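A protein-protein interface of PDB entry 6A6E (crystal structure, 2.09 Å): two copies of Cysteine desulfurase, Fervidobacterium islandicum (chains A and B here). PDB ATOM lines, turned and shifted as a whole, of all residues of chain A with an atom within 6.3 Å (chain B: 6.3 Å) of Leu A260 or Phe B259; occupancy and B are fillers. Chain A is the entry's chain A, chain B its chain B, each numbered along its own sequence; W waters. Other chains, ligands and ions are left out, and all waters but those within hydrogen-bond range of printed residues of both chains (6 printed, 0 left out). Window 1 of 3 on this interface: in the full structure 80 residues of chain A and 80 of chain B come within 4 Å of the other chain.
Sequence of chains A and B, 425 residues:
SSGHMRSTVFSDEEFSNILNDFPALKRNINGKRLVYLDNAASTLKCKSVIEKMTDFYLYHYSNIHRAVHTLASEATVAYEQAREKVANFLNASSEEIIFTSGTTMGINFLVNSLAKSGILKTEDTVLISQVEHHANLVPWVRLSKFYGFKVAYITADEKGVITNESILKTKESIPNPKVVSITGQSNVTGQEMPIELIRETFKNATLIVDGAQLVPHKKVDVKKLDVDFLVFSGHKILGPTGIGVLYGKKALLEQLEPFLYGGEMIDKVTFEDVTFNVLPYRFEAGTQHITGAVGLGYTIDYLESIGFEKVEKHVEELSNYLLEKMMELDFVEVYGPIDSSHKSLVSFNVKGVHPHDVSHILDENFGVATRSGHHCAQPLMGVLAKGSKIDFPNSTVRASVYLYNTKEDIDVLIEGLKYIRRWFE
O of Tyr B261 is in hydrogen-bond range of ND2 of Asn A108, at 2.8 Å.
O of Tyr A261 is in hydrogen-bond range of ND2 of Asn B108, 2.8 Å away.
Asn A108 touches Leu B260 (OD1 to CA, 3.5 Å).
Tyr B261 touches Leu A143 (CE2 to CG, 3.7 Å).
CZ of Phe B259 touches CZ of Phe A259 (3.6 Å).
Phe A259 touches Leu B260 (CZ to CD2, 3.8 Å).
OD1 of Asn B108 touches CA of Leu A260 (3.6 Å).
Leu A260 touches Phe B259 (CD2 to CZ, 3.8 Å).
Tyr A261 touches Thr B104 (O to CG2, 3.4 Å).
Ala A285 touches Thr B104 (O to CG2, 3.8 Å).
O of Phe A259 lies within hydrogen-bond range of NZ of Lys A116.
The backbone carbonyl oxygen of Thr B104 is in hydrogen-bond range of the side-chain amide nitrogen of Asn B108, 2.9 Å away.
The backbone carbonyl oxygen of Phe B259 lies within hydrogen-bond range of the side-chain amino group of Lys B116 (3.0 Å).
OH of Tyr B261 lies within hydrogen-bond range of NZ of Lys B116 (3.0 Å).
OH of Tyr B261 lies within hydrogen-bond range of OE2 of Glu B257 (2.6 Å).
Of the printed residues of chain B, Leu A260 touches Asn B108 (3.6 Å) and Phe B259 (3.8 Å).
Of the printed residues of chain A, Tyr B261 touches Asn A108 and Leu A143.
Of the printed residues of chain B, Tyr A261 touches Thr B104 (3.4 Å) and Asn B108 (2.8 Å).
Printed residues of chain B within 4 Å of Phe A259: Phe B259 (3.6 Å) and Leu B260 (3.8 Å).
Ser B101 touches none of the printed residues of chain A.
Pro B258 touches none of the printed residues of chain A.
The nearest residue of chain A that does not touch Phe B259 is Asn A108 (4.4 Å).
The nearest printed residue of chain A that does not touch Tyr B261 is Asn A112 (6.0 Å).
Printed residues of chain A that touch a printed residue of chain B: Asn A108, Leu A143, Phe A259, Leu A260, Tyr A261 and Ala A285.
Printed residues of chain B that touch a printed residue of chain A: Thr B104, Asn B108, Phe B259, Leu B260 and Tyr B261.
Hydrophobic or aromatic side chains of chain B within 4 Å of the printed part of chain A: Phe B259, Leu B260 and Tyr B261.
Among the printed residues, 10 pairs touch across the chains.
Water W2 lies within hydrogen-bond range of the side-chain hydroxyl of Ser B101 (2.7 Å) and the side-chain sulfur of Met A105 (3.8 Å).
Water W5 lies within hydrogen-bond range of the side-chain amide oxygen (OD1) of Asn B112 and the side-chain amino group (NZ) of Lys A116.
Water W1 lies within hydrogen-bond range of the side-chain amide oxygen of Asn A108 (2.8 Å), the backbone carbonyl oxygen of Phe B259 (2.8 Å) and the side-chain amide nitrogen of Asn A112 (2.8 Å).
Water W3 lies within hydrogen-bond range of SD of Met B105 (2.8 Å), OG of Ser B101 (2.9 Å) and SD of Met A105 (3.1 Å).
Asn A108 touches Leu B260, and with the chains exchanged Leu A260 touches Asn B108.
Asn A108 touches Tyr B261, and with the chains exchanged Tyr A261 touches Asn B108.
Phe B259 touches its own counterpart, Phe A259.
Phe A259 touches Leu B260, and with the chains exchanged Leu A260 touches Phe B259.
Positions printed for both chains: 105, 108, 109, 112, 113, 116, 258, 259, 260, 261, 265, 282 and 283.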
ATOM      1  N   MET A 105     -11.061  21.349  -6.213  1.00  0.00           N
ATOM      2  CA  MET A 105     -11.267  20.120  -7.007  1.00  0.00           C
ATOM      3  C   MET A 105      -9.947  19.580  -7.558  1.00  0.00           C
ATOM      4  O   MET A 105      -9.680  18.386  -7.515  1.00  0.00           O
ATOM      5  CB  MET A 105     -12.266  20.332  -8.171  1.00  0.00           C
ATOM      6  CG  MET A 105     -12.174  19.222  -9.251  1.00  0.00           C
ATOM      7  SD  MET A 105     -13.506  19.227 -10.473  1.00  0.00           S
ATOM      8  CE  MET A 105     -12.830  18.171 -11.794  1.00  0.00           C
ATOM      9  N   ASN A 108      -8.042  17.685  -4.951  1.00  0.00           N
ATOM     10  CA  ASN A 108      -8.704  16.397  -4.702  1.00  0.00           C
ATOM     11  C   ASN A 108      -8.447  15.410  -5.856  1.00  0.00           C
ATOM     12  O   ASN A 108      -8.250  14.213  -5.612  1.00  0.00           O
ATOM     13  CB  ASN A 108     -10.211  16.578  -4.473  1.00  0.00           C
ATOM     14  CG  ASN A 108     -10.534  17.036  -3.068  1.00  0.00           C
ATOM     15  OD1 ASN A 108     -10.742  16.197  -2.167  1.00  0.00           O
ATOM     16  ND2 ASN A 108     -10.550  18.366  -2.841  1.00  0.00           N
ATOM     17  N   PHE A 109      -8.478  15.917  -7.091  1.00  0.00           N
ATOM     18  CA  PHE A 109      -8.224  15.146  -8.291  1.00  0.00           C
ATOM     19  C   PHE A 109      -6.827  14.478  -8.144  1.00  0.00           C
ATOM     20  O   PHE A 109      -6.661  13.256  -8.362  1.00  0.00           O
ATOM     21  CB  PHE A 109      -8.333  16.094  -9.469  1.00  0.00           C
ATOM     22  CG  PHE A 109      -7.914  15.565 -10.814  1.00  0.00           C
ATOM     23  CD1 PHE A 109      -6.699  14.908 -11.028  1.00  0.00           C
ATOM     24  CD2 PHE A 109      -8.678  15.897 -11.923  1.00  0.00           C
ATOM     25  CE1 PHE A 109      -6.309  14.489 -12.297  1.00  0.00           C
ATOM     26  CE2 PHE A 109      -8.292  15.492 -13.203  1.00  0.00           C
ATOM     27  CZ  PHE A 109      -7.111  14.759 -13.374  1.00  0.00           C
ATOM     28  N   ASN A 112      -6.535  11.619  -5.191  1.00  0.00           N
ATOM     29  CA  ASN A 112      -7.230  10.439  -5.591  1.00  0.00           C
ATOM     30  C   ASN A 112      -6.585   9.792  -6.818  1.00  0.00           C
ATOM     31  O   ASN A 112      -6.483   8.517  -6.863  1.00  0.00           O
ATOM     32  CB  ASN A 112      -8.736  10.660  -5.860  1.00  0.00           C
ATOM     33  CG  ASN A 112      -9.504  10.948  -4.635  1.00  0.00           C
ATOM     34  OD1 ASN A 112      -9.922  10.018  -3.928  1.00  0.00           O
ATOM     35  ND2 ASN A 112      -9.736  12.273  -4.349  1.00  0.00           N
ATOM     36  N   SER A 113      -6.247  10.575  -7.843  1.00  0.00           N
ATOM     37  CA  SER A 113      -5.651   9.974  -9.021  1.00  0.00           C
ATOM     38  C   SER A 113      -4.240   9.409  -8.687  1.00  0.00           C
ATOM     39  O   SER A 113      -3.900   8.333  -9.156  1.00  0.00           O
ATOM     40  CB  SER A 113      -5.544  10.905 -10.228  1.00  0.00           C
ATOM     41  OG  SER A 113      -6.892  11.267 -10.662  1.00  0.00           O
ATOM     42  N   LYS A 116      -4.860   5.986  -7.007  1.00  0.00           N
ATOM     43  CA  LYS A 116      -5.437   4.981  -7.879  1.00  0.00           C
ATOM     44  C   LYS A 116      -4.503   4.543  -8.952  1.00  0.00           C
ATOM     45  O   LYS A 116      -4.688   3.492  -9.505  1.00  0.00           O
ATOM     46  CB  LYS A 116      -6.741   5.492  -8.563  1.00  0.00           C
ATOM     47  CG  LYS A 116      -7.963   5.655  -7.640  1.00  0.00           C
ATOM     48  CD  LYS A 116      -9.289   5.796  -8.462  1.00  0.00           C
ATOM     49  CE  LYS A 116      -9.464   7.163  -9.193  1.00  0.00           C
ATOM     50  NZ  LYS A 116     -10.838   7.529  -9.821  1.00  0.00           N
ATOM     51  N   LEU A 143      -7.577  11.719   3.405  1.00  0.00           N
ATOM     52  CA  LEU A 143      -7.390  10.563   2.581  1.00  0.00           C
ATOM     53  C   LEU A 143      -6.229   9.625   3.011  1.00  0.00           C
ATOM     54  O   LEU A 143      -6.268   8.418   2.650  1.00  0.00           O
ATOM     55  CB  LEU A 143      -7.355  10.861   1.098  1.00  0.00           C
ATOM     56  CG  LEU A 143      -8.671  11.361   0.465  1.00  0.00           C
ATOM     57  CD1 LEU A 143      -8.349  11.919  -0.900  1.00  0.00           C
ATOM     58  CD2 LEU A 143      -9.716  10.288   0.372  1.00  0.00           C
ATOM     59  N   PRO A 258      -7.960   8.496 -14.475  1.00  0.00           N
ATOM     60  CA  PRO A 258      -8.864   9.689 -14.379  1.00  0.00           C
ATOM     61  C   PRO A 258      -9.419   9.767 -12.989  1.00  0.00           C
ATOM     62  O   PRO A 258      -9.650   8.720 -12.343  1.00  0.00           O
ATOM     63  CB  PRO A 258      -9.950   9.385 -15.382  1.00  0.00           C
ATOM     64  CG  PRO A 258      -9.248   8.525 -16.452  1.00  0.00           C
ATOM     65  CD  PRO A 258      -8.248   7.687 -15.674  1.00  0.00           C
ATOM     66  N   PHE A 259      -9.665  10.982 -12.518  1.00  0.00           N
ATOM     67  CA  PHE A 259     -10.359  11.173 -11.246  1.00  0.00           C
ATOM     68  C   PHE A 259     -11.894  10.825 -11.369  1.00  0.00           C
ATOM     69  O   PHE A 259     -12.405   9.947 -10.701  1.00  0.00           O
ATOM     70  CB  PHE A 259     -10.138  12.653 -10.772  1.00  0.00           C
ATOM     71  CG  PHE A 259     -10.761  12.975  -9.497  1.00  0.00           C
ATOM     72  CD1 PHE A 259     -10.916  12.007  -8.530  1.00  0.00           C
ATOM     73  CD2 PHE A 259     -11.300  14.238  -9.281  1.00  0.00           C
ATOM     74  CE1 PHE A 259     -11.514  12.286  -7.322  1.00  0.00           C
ATOM     75  CE2 PHE A 259     -11.875  14.538  -8.051  1.00  0.00           C
ATOM     76  CZ  PHE A 259     -11.968  13.572  -7.093  1.00  0.00           C
ATOM     77  N   LEU A 260     -12.589  11.567 -12.203  1.00  0.00           N
ATOM     78  CA  LEU A 260     -13.970  11.401 -12.510  1.00  0.00           C
ATOM     79  C   LEU A 260     -14.177  10.680 -13.847  1.00  0.00           C
ATOM     80  O   LEU A 260     -13.368  10.833 -14.800  1.00  0.00           O
ATOM     81  CB  LEU A 260     -14.649  12.764 -12.621  1.00  0.00           C
ATOM     82  CG  LEU A 260     -14.476  13.757 -11.466  1.00  0.00           C
ATOM     83  CD1 LEU A 260     -15.261  15.062 -11.678  1.00  0.00           C
ATOM     84  CD2 LEU A 260     -14.839  13.076 -10.189  1.00  0.00           C
ATOM     85  N   TYR A 261     -15.329   9.983 -13.935  1.00  0.00           N
ATOM     86  CA  TYR A 261     -15.718   9.246 -15.120  1.00  0.00           C
ATOM     87  C   TYR A 261     -17.065   9.619 -15.634  1.00  0.00           C
ATOM     88  O   TYR A 261     -17.910  10.038 -14.875  1.00  0.00           O
ATOM     89  CB  TYR A 261     -15.783   7.772 -14.738  1.00  0.00           C
ATOM     90  CG  TYR A 261     -14.558   7.241 -14.040  1.00  0.00           C
ATOM     91  CD1 TYR A 261     -13.449   6.847 -14.756  1.00  0.00           C
ATOM     92  CD2 TYR A 261     -14.549   7.078 -12.642  1.00  0.00           C
ATOM     93  CE1 TYR A 261     -12.322   6.332 -14.096  1.00  0.00           C
ATOM     94  CE2 TYR A 261     -13.437   6.572 -11.983  1.00  0.00           C
ATOM     95  CZ  TYR A 261     -12.357   6.167 -12.698  1.00  0.00           C
ATOM     96  OH  TYR A 261     -11.256   5.672 -11.981  1.00  0.00           O
ATOM     97  N   GLY A 262     -17.256   9.458 -16.939  1.00  0.00           N
ATOM     98  CA  GLY A 262     -18.500   9.777 -17.592  1.00  0.00           C
ATOM     99  C   GLY A 262     -18.261   9.991 -19.070  1.00  0.00           C
ATOM    100  O   GLY A 262     -17.334   9.434 -19.675  1.00  0.00           O
ATOM    101  N   MET A 265     -14.743  11.694 -21.733  1.00  0.00           N
ATOM    102  CA  MET A 265     -13.452  11.206 -21.315  1.00  0.00           C
ATOM    103  C   MET A 265     -13.165   9.754 -21.714  1.00  0.00           C
ATOM    104  O   MET A 265     -12.041   9.274 -21.517  1.00  0.00           O
ATOM    105  CB  MET A 265     -13.241  11.411 -19.808  1.00  0.00           C
ATOM    106  CG  MET A 265     -14.234  10.760 -18.874  1.00  0.00           C
ATOM    107  SD  MET A 265     -14.061   8.991 -18.539  1.00  0.00           S
ATOM    108  CE  MET A 265     -12.481   9.081 -17.676  1.00  0.00           C
ATOM    109  N   ARG A 282      -9.409  13.103 -21.667  1.00  0.00           N
ATOM    110  CA  ARG A 282      -9.358  12.074 -20.632  1.00  0.00           C
ATOM    111  C   ARG A 282      -9.742  12.504 -19.219  1.00  0.00           C
ATOM    112  O   ARG A 282     -10.257  11.668 -18.421  1.00  0.00           O
ATOM    113  CB  ARG A 282      -7.947  11.480 -20.601  1.00  0.00           C
ATOM    114  CG  ARG A 282      -7.719  10.425 -19.560  1.00  0.00           C
ATOM    115  CD  ARG A 282      -6.277   9.876 -19.655  1.00  0.00           C
ATOM    116  NE  ARG A 282      -6.156   9.299 -20.960  1.00  0.00           N
ATOM    117  CZ  ARG A 282      -5.032   8.878 -21.522  1.00  0.00           C
ATOM    118  NH1 ARG A 282      -3.849   8.952 -20.887  1.00  0.00           N
ATOM    119  NH2 ARG A 282      -5.120   8.391 -22.752  1.00  0.00           N
ATOM    120  N   PHE A 283      -9.442  13.759 -18.872  1.00  0.00           N
ATOM    121  CA  PHE A 283      -9.632  14.248 -17.525  1.00  0.00           C
ATOM    122  C   PHE A 283     -10.771  15.257 -17.382  1.00  0.00           C
ATOM    123  O   PHE A 283     -10.885  15.892 -16.332  1.00  0.00           O
ATOM    124  CB  PHE A 283      -8.330  14.831 -16.974  1.00  0.00           C
ATOM    125  CG  PHE A 283      -7.215  13.828 -16.950  1.00  0.00           C
ATOM    126  CD1 PHE A 283      -7.278  12.780 -16.091  1.00  0.00           C
ATOM    127  CD2 PHE A 283      -6.187  13.878 -17.861  1.00  0.00           C
ATOM    128  CE1 PHE A 283      -6.309  11.823 -16.060  1.00  0.00           C
ATOM    129  CE2 PHE A 283      -5.184  12.913 -17.849  1.00  0.00           C
ATOM    130  CZ  PHE A 283      -5.249  11.870 -16.943  1.00  0.00           C
ATOM    131  N   GLU A 284     -11.606  15.341 -18.417  1.00  0.00           N
ATOM    132  CA  GLU A 284     -12.869  16.115 -18.420  1.00  0.00           C
ATOM    133  C   GLU A 284     -14.119  15.247 -18.592  1.00  0.00           C
ATOM    134  O   GLU A 284     -14.448  14.872 -19.672  1.00  0.00           O
ATOM    135  CB  GLU A 284     -12.807  17.220 -19.492  1.00  0.00           C
ATOM    136  CG  GLU A 284     -11.743  18.276 -19.108  1.00  0.00           C
ATOM    137  CD  GLU A 284     -11.521  19.442 -20.088  1.00  0.00           C
ATOM    138  OE1 GLU A 284     -12.301  19.618 -21.073  1.00  0.00           O
ATOM    139  OE2 GLU A 284     -10.600  20.250 -19.799  1.00  0.00           O
ATOM    140  N   ALA A 285     -14.749  14.899 -17.478  1.00  0.00           N
ATOM    141  CA  ALA A 285     -15.903  14.043 -17.439  1.00  0.00           C
ATOM    142  C   ALA A 285     -17.190  14.836 -17.485  1.00  0.00           C
ATOM    143  O   ALA A 285     -17.417  15.694 -16.646  1.00  0.00           O
ATOM    144  CB  ALA A 285     -15.845  13.142 -16.204  1.00  0.00           C
ATOM    145  N   SER B 101     -20.941  20.486  -9.747  1.00  0.00           N
ATOM    146  CA  SER B 101     -20.633  20.955 -11.116  1.00  0.00           C
ATOM    147  C   SER B 101     -21.557  20.379 -12.198  1.00  0.00           C
ATOM    148  O   SER B 101     -21.527  20.859 -13.299  1.00  0.00           O
ATOM    149  CB  SER B 101     -19.214  20.674 -11.463  1.00  0.00           C
ATOM    150  OG  SER B 101     -18.977  19.272 -11.537  1.00  0.00           O
ATOM    151  N   THR B 104     -22.833  14.617 -13.798  1.00  0.00           N
ATOM    152  CA  THR B 104     -21.727  13.672 -13.856  1.00  0.00           C
ATOM    153  C   THR B 104     -20.946  13.677 -12.515  1.00  0.00           C
ATOM    154  O   THR B 104     -20.682  12.600 -11.938  1.00  0.00           O
ATOM    155  CB  THR B 104     -20.791  13.931 -15.029  1.00  0.00           C
ATOM    156  OG1 THR B 104     -21.523  13.832 -16.261  1.00  0.00           O
ATOM    157  CG2 THR B 104     -19.622  12.985 -15.084  1.00  0.00           C
ATOM    158  N   MET B 105     -20.610  14.841 -12.025  1.00  0.00           N
ATOM    159  CA  MET B 105     -19.916  14.921 -10.738  1.00  0.00           C
ATOM    160  C   MET B 105     -20.777  14.309  -9.657  1.00  0.00           C
ATOM    161  O   MET B 105     -20.284  13.639  -8.768  1.00  0.00           O
ATOM    162  CB  MET B 105     -19.600  16.350 -10.320  1.00  0.00           C
ATOM    163  CG  MET B 105     -19.106  16.466  -8.862  1.00  0.00           C
ATOM    164  SD  MET B 105     -18.738  18.194  -8.447  1.00  0.00           S
ATOM    165  CE  MET B 105     -18.824  18.051  -6.627  1.00  0.00           C
ATOM    166  N   ASN B 108     -20.495  10.480  -9.654  1.00  0.00           N
ATOM    167  CA  ASN B 108     -19.142  10.144  -9.195  1.00  0.00           C
ATOM    168  C   ASN B 108     -19.064  10.357  -7.705  1.00  0.00           C
ATOM    169  O   ASN B 108     -18.522   9.555  -6.992  1.00  0.00           O
ATOM    170  CB  ASN B 108     -18.046  10.972  -9.910  1.00  0.00           C
ATOM    171  CG  ASN B 108     -17.713  10.435 -11.265  1.00  0.00           C
ATOM    172  OD1 ASN B 108     -16.824   9.576 -11.384  1.00  0.00           O
ATOM    173  ND2 ASN B 108     -18.406  10.920 -12.305  1.00  0.00           N
ATOM    174  N   PHE B 109     -19.681  11.410  -7.205  1.00  0.00           N
ATOM    175  CA  PHE B 109     -19.739  11.638  -5.756  1.00  0.00           C
ATOM    176  C   PHE B 109     -20.366  10.435  -5.031  1.00  0.00           C
ATOM    177  O   PHE B 109     -19.871   9.981  -3.990  1.00  0.00           O
ATOM    178  CB  PHE B 109     -20.517  12.946  -5.541  1.00  0.00           C
ATOM    179  CG  PHE B 109     -20.948  13.243  -4.146  1.00  0.00           C
ATOM    180  CD1 PHE B 109     -21.581  12.326  -3.344  1.00  0.00           C
ATOM    181  CD2 PHE B 109     -20.903  14.544  -3.723  1.00  0.00           C
ATOM    182  CE1 PHE B 109     -22.079  12.661  -2.099  1.00  0.00           C
ATOM    183  CE2 PHE B 109     -21.404  14.884  -2.473  1.00  0.00           C
ATOM    184  CZ  PHE B 109     -21.982  13.934  -1.661  1.00  0.00           C
ATOM    185  N   LEU B 110     -21.507   9.996  -5.526  1.00  0.00           N
ATOM    186  CA  LEU B 110     -22.234   8.931  -4.904  1.00  0.00           C
ATOM    187  C   LEU B 110     -21.431   7.607  -4.919  1.00  0.00           C
ATOM    188  O   LEU B 110     -21.387   6.907  -3.912  1.00  0.00           O
ATOM    189  CB  LEU B 110     -23.621   8.754  -5.530  1.00  0.00           C
ATOM    190  CG  LEU B 110     -24.590   9.888  -5.200  1.00  0.00           C
ATOM    191  CD1 LEU B 110     -25.840   9.807  -6.006  1.00  0.00           C
ATOM    192  CD2 LEU B 110     -24.927   9.971  -3.735  1.00  0.00           C
ATOM    193  N   ASN B 112     -18.097   7.016  -5.131  1.00  0.00           N
ATOM    194  CA  ASN B 112     -16.965   7.103  -4.204  1.00  0.00           C
ATOM    195  C   ASN B 112     -17.425   7.192  -2.753  1.00  0.00           C
ATOM    196  O   ASN B 112     -16.908   6.470  -1.854  1.00  0.00           O
ATOM    197  CB  ASN B 112     -16.087   8.303  -4.549  1.00  0.00           C
ATOM    198  CG  ASN B 112     -15.328   8.105  -5.808  1.00  0.00           C
ATOM    199  OD1 ASN B 112     -14.349   7.426  -5.771  1.00  0.00           O
ATOM    200  ND2 ASN B 112     -15.783   8.683  -6.954  1.00  0.00           N
ATOM    201  N   SER B 113     -18.413   8.040  -2.490  1.00  0.00           N
ATOM    202  CA  SER B 113     -18.875   8.171  -1.153  1.00  0.00           C
ATOM    203  C   SER B 113     -19.583   6.913  -0.566  1.00  0.00           C
ATOM    204  O   SER B 113     -19.408   6.587   0.650  1.00  0.00           O
ATOM    205  CB  SER B 113     -19.748   9.387  -1.016  1.00  0.00           C
ATOM    206  OG  SER B 113     -20.149   9.547   0.344  1.00  0.00           O
ATOM    207  N   LYS B 116     -16.625   4.577   0.147  1.00  0.00           N
ATOM    208  CA  LYS B 116     -15.805   4.998   1.270  1.00  0.00           C
ATOM    209  C   LYS B 116     -16.557   4.868   2.584  1.00  0.00           C
ATOM    210  O   LYS B 116     -15.910   4.803   3.609  1.00  0.00           O
ATOM    211  CB  LYS B 116     -15.318   6.481   1.175  1.00  0.00           C
ATOM    212  CG  LYS B 116     -14.181   6.764   0.196  1.00  0.00           C
ATOM    213  CD  LYS B 116     -13.506   8.137   0.457  1.00  0.00           C
ATOM    214  CE  LYS B 116     -14.371   9.335  -0.013  1.00  0.00           C
ATOM    215  NZ  LYS B 116     -13.633  10.620  -0.393  1.00  0.00           N
ATOM    216  N   GLU B 257     -19.603   9.584   4.013  1.00  0.00           N
ATOM    217  CA  GLU B 257     -18.303  10.293   3.989  1.00  0.00           C
ATOM    218  C   GLU B 257     -18.288  11.343   2.863  1.00  0.00           C
ATOM    219  O   GLU B 257     -18.721  11.066   1.736  1.00  0.00           O
ATOM    220  CB  GLU B 257     -17.225   9.276   3.715  1.00  0.00           C
ATOM    221  CG  GLU B 257     -15.817   9.784   3.538  1.00  0.00           C
ATOM    222  CD  GLU B 257     -15.134  10.316   4.777  1.00  0.00           C
ATOM    223  OE1 GLU B 257     -15.615  10.003   5.861  1.00  0.00           O
ATOM    224  OE2 GLU B 257     -14.094  11.047   4.682  1.00  0.00           O
ATOM    225  N   PRO B 258     -17.706  12.501   3.093  1.00  0.00           N
ATOM    226  CA  PRO B 258     -17.713  13.477   1.966  1.00  0.00           C
ATOM    227  C   PRO B 258     -16.884  12.945   0.786  1.00  0.00           C
ATOM    228  O   PRO B 258     -15.943  12.150   1.000  1.00  0.00           O
ATOM    229  CB  PRO B 258     -17.092  14.692   2.575  1.00  0.00           C
ATOM    230  CG  PRO B 258     -17.461  14.607   4.032  1.00  0.00           C
ATOM    231  CD  PRO B 258     -17.308  13.129   4.357  1.00  0.00           C
ATOM    232  N   PHE B 259     -17.225  13.327  -0.445  1.00  0.00           N
ATOM    233  CA  PHE B 259     -16.422  12.939  -1.618  1.00  0.00           C
ATOM    234  C   PHE B 259     -15.154  13.783  -1.714  1.00  0.00           C
ATOM    235  O   PHE B 259     -14.018  13.266  -1.689  1.00  0.00           O
ATOM    236  CB  PHE B 259     -17.304  13.095  -2.900  1.00  0.00           C
ATOM    237  CG  PHE B 259     -16.594  12.780  -4.167  1.00  0.00           C
ATOM    238  CD1 PHE B 259     -15.590  11.846  -4.198  1.00  0.00           C
ATOM    239  CD2 PHE B 259     -16.919  13.427  -5.323  1.00  0.00           C
ATOM    240  CE1 PHE B 259     -14.904  11.560  -5.381  1.00  0.00           C
ATOM    241  CE2 PHE B 259     -16.264  13.161  -6.509  1.00  0.00           C
ATOM    242  CZ  PHE B 259     -15.257  12.233  -6.548  1.00  0.00           C
ATOM    243  N   LEU B 260     -15.349  15.109  -1.737  1.00  0.00           N
ATOM    244  CA  LEU B 260     -14.244  16.102  -1.846  1.00  0.00           C
ATOM    245  C   LEU B 260     -13.967  16.781  -0.497  1.00  0.00           C
ATOM    246  O   LEU B 260     -14.902  16.993   0.258  1.00  0.00           O
ATOM    247  CB  LEU B 260     -14.648  17.192  -2.819  1.00  0.00           C
ATOM    248  CG  LEU B 260     -15.014  16.802  -4.252  1.00  0.00           C
ATOM    249  CD1 LEU B 260     -15.164  17.991  -5.184  1.00  0.00           C
ATOM    250  CD2 LEU B 260     -13.944  15.899  -4.830  1.00  0.00           C
ATOM    251  N   TYR B 261     -12.714  17.154  -0.223  1.00  0.00           N
ATOM    252  CA  TYR B 261     -12.325  17.841   0.981  1.00  0.00           C
ATOM    253  C   TYR B 261     -11.701  19.190   0.710  1.00  0.00           C
ATOM    254  O   TYR B 261     -11.072  19.393  -0.301  1.00  0.00           O
ATOM    255  CB  TYR B 261     -11.311  16.999   1.782  1.00  0.00           C
ATOM    256  CG  TYR B 261     -11.772  15.565   1.963  1.00  0.00           C
ATOM    257  CD1 TYR B 261     -12.580  15.211   3.017  1.00  0.00           C
ATOM    258  CD2 TYR B 261     -11.379  14.595   1.082  1.00  0.00           C
ATOM    259  CE1 TYR B 261     -13.024  13.909   3.156  1.00  0.00           C
ATOM    260  CE2 TYR B 261     -11.764  13.282   1.223  1.00  0.00           C
ATOM    261  CZ  TYR B 261     -12.580  12.936   2.268  1.00  0.00           C
ATOM    262  OH  TYR B 261     -12.958  11.607   2.409  1.00  0.00           O
ATOM    263  N   MET B 265     -16.391  22.857   4.068  1.00  0.00           N
ATOM    264  CA  MET B 265     -16.937  21.543   4.432  1.00  0.00           C
ATOM    265  C   MET B 265     -16.413  20.977   5.750  1.00  0.00           C
ATOM    266  O   MET B 265     -16.974  20.006   6.216  1.00  0.00           O
ATOM    267  CB  MET B 265     -16.736  20.520   3.329  1.00  0.00           C
ATOM    268  CG  MET B 265     -15.305  20.214   2.909  1.00  0.00           C
ATOM    269  SD  MET B 265     -14.421  19.031   3.943  1.00  0.00           S
ATOM    270  CE  MET B 265     -15.336  17.554   3.656  1.00  0.00           C
ATOM    271  N   ARG B 282     -21.159  20.134   4.425  1.00  0.00           N
ATOM    272  CA  ARG B 282     -20.331  18.925   4.497  1.00  0.00           C
ATOM    273  C   ARG B 282     -19.895  18.425   3.119  1.00  0.00           C
ATOM    274  O   ARG B 282     -18.794  17.783   2.933  1.00  0.00           O
ATOM    275  CB  ARG B 282     -21.243  17.859   5.135  1.00  0.00           C
ATOM    276  CG  ARG B 282     -20.609  16.507   5.407  1.00  0.00           C
ATOM    277  CD  ARG B 282     -21.471  15.788   6.440  1.00  0.00           C
ATOM    278  NE  ARG B 282     -20.653  14.813   7.149  1.00  0.00           N
ATOM    279  CZ  ARG B 282     -20.844  13.490   7.146  1.00  0.00           C
ATOM    280  NH1 ARG B 282     -19.976  12.695   7.772  1.00  0.00           N
ATOM    281  NH2 ARG B 282     -21.910  12.941   6.543  1.00  0.00           N
ATOM    282  N   PHE B 283     -20.790  18.629   2.153  1.00  0.00           N
ATOM    283  CA  PHE B 283     -20.569  18.136   0.790  1.00  0.00           C
ATOM    284  C   PHE B 283     -20.242  19.207  -0.276  1.00  0.00           C
ATOM    285  O   PHE B 283     -20.291  18.902  -1.440  1.00  0.00           O
ATOM    286  CB  PHE B 283     -21.755  17.250   0.343  1.00  0.00           C
ATOM    287  CG  PHE B 283     -22.033  16.126   1.283  1.00  0.00           C
ATOM    288  CD1 PHE B 283     -21.140  15.078   1.400  1.00  0.00           C
ATOM    289  CD2 PHE B 283     -23.104  16.167   2.126  1.00  0.00           C
ATOM    290  CE1 PHE B 283     -21.334  14.093   2.314  1.00  0.00           C
ATOM    291  CE2 PHE B 283     -23.329  15.140   3.029  1.00  0.00           C
ATOM    292  CZ  PHE B 283     -22.455  14.093   3.098  1.00  0.00           C
HETATM  293  O   HOH W   1     -11.331  13.514  -2.392  1.00  0.00           O
HETATM  294  O   HOH W   2     -16.616  18.417 -12.409  1.00  0.00           O
HETATM  295  O   HOH W   3     -16.558  19.083 -10.041  1.00  0.00           O
HETATM  296  O   HOH W   4     -14.791   8.882  -9.605  1.00  0.00           O
HETATM  297  O   HOH W   5     -12.010   7.696  -7.121  1.00  0.00           O
HETATM  298  O   HOH W   6     -12.215   9.801  -2.368  1.00  0.00           O
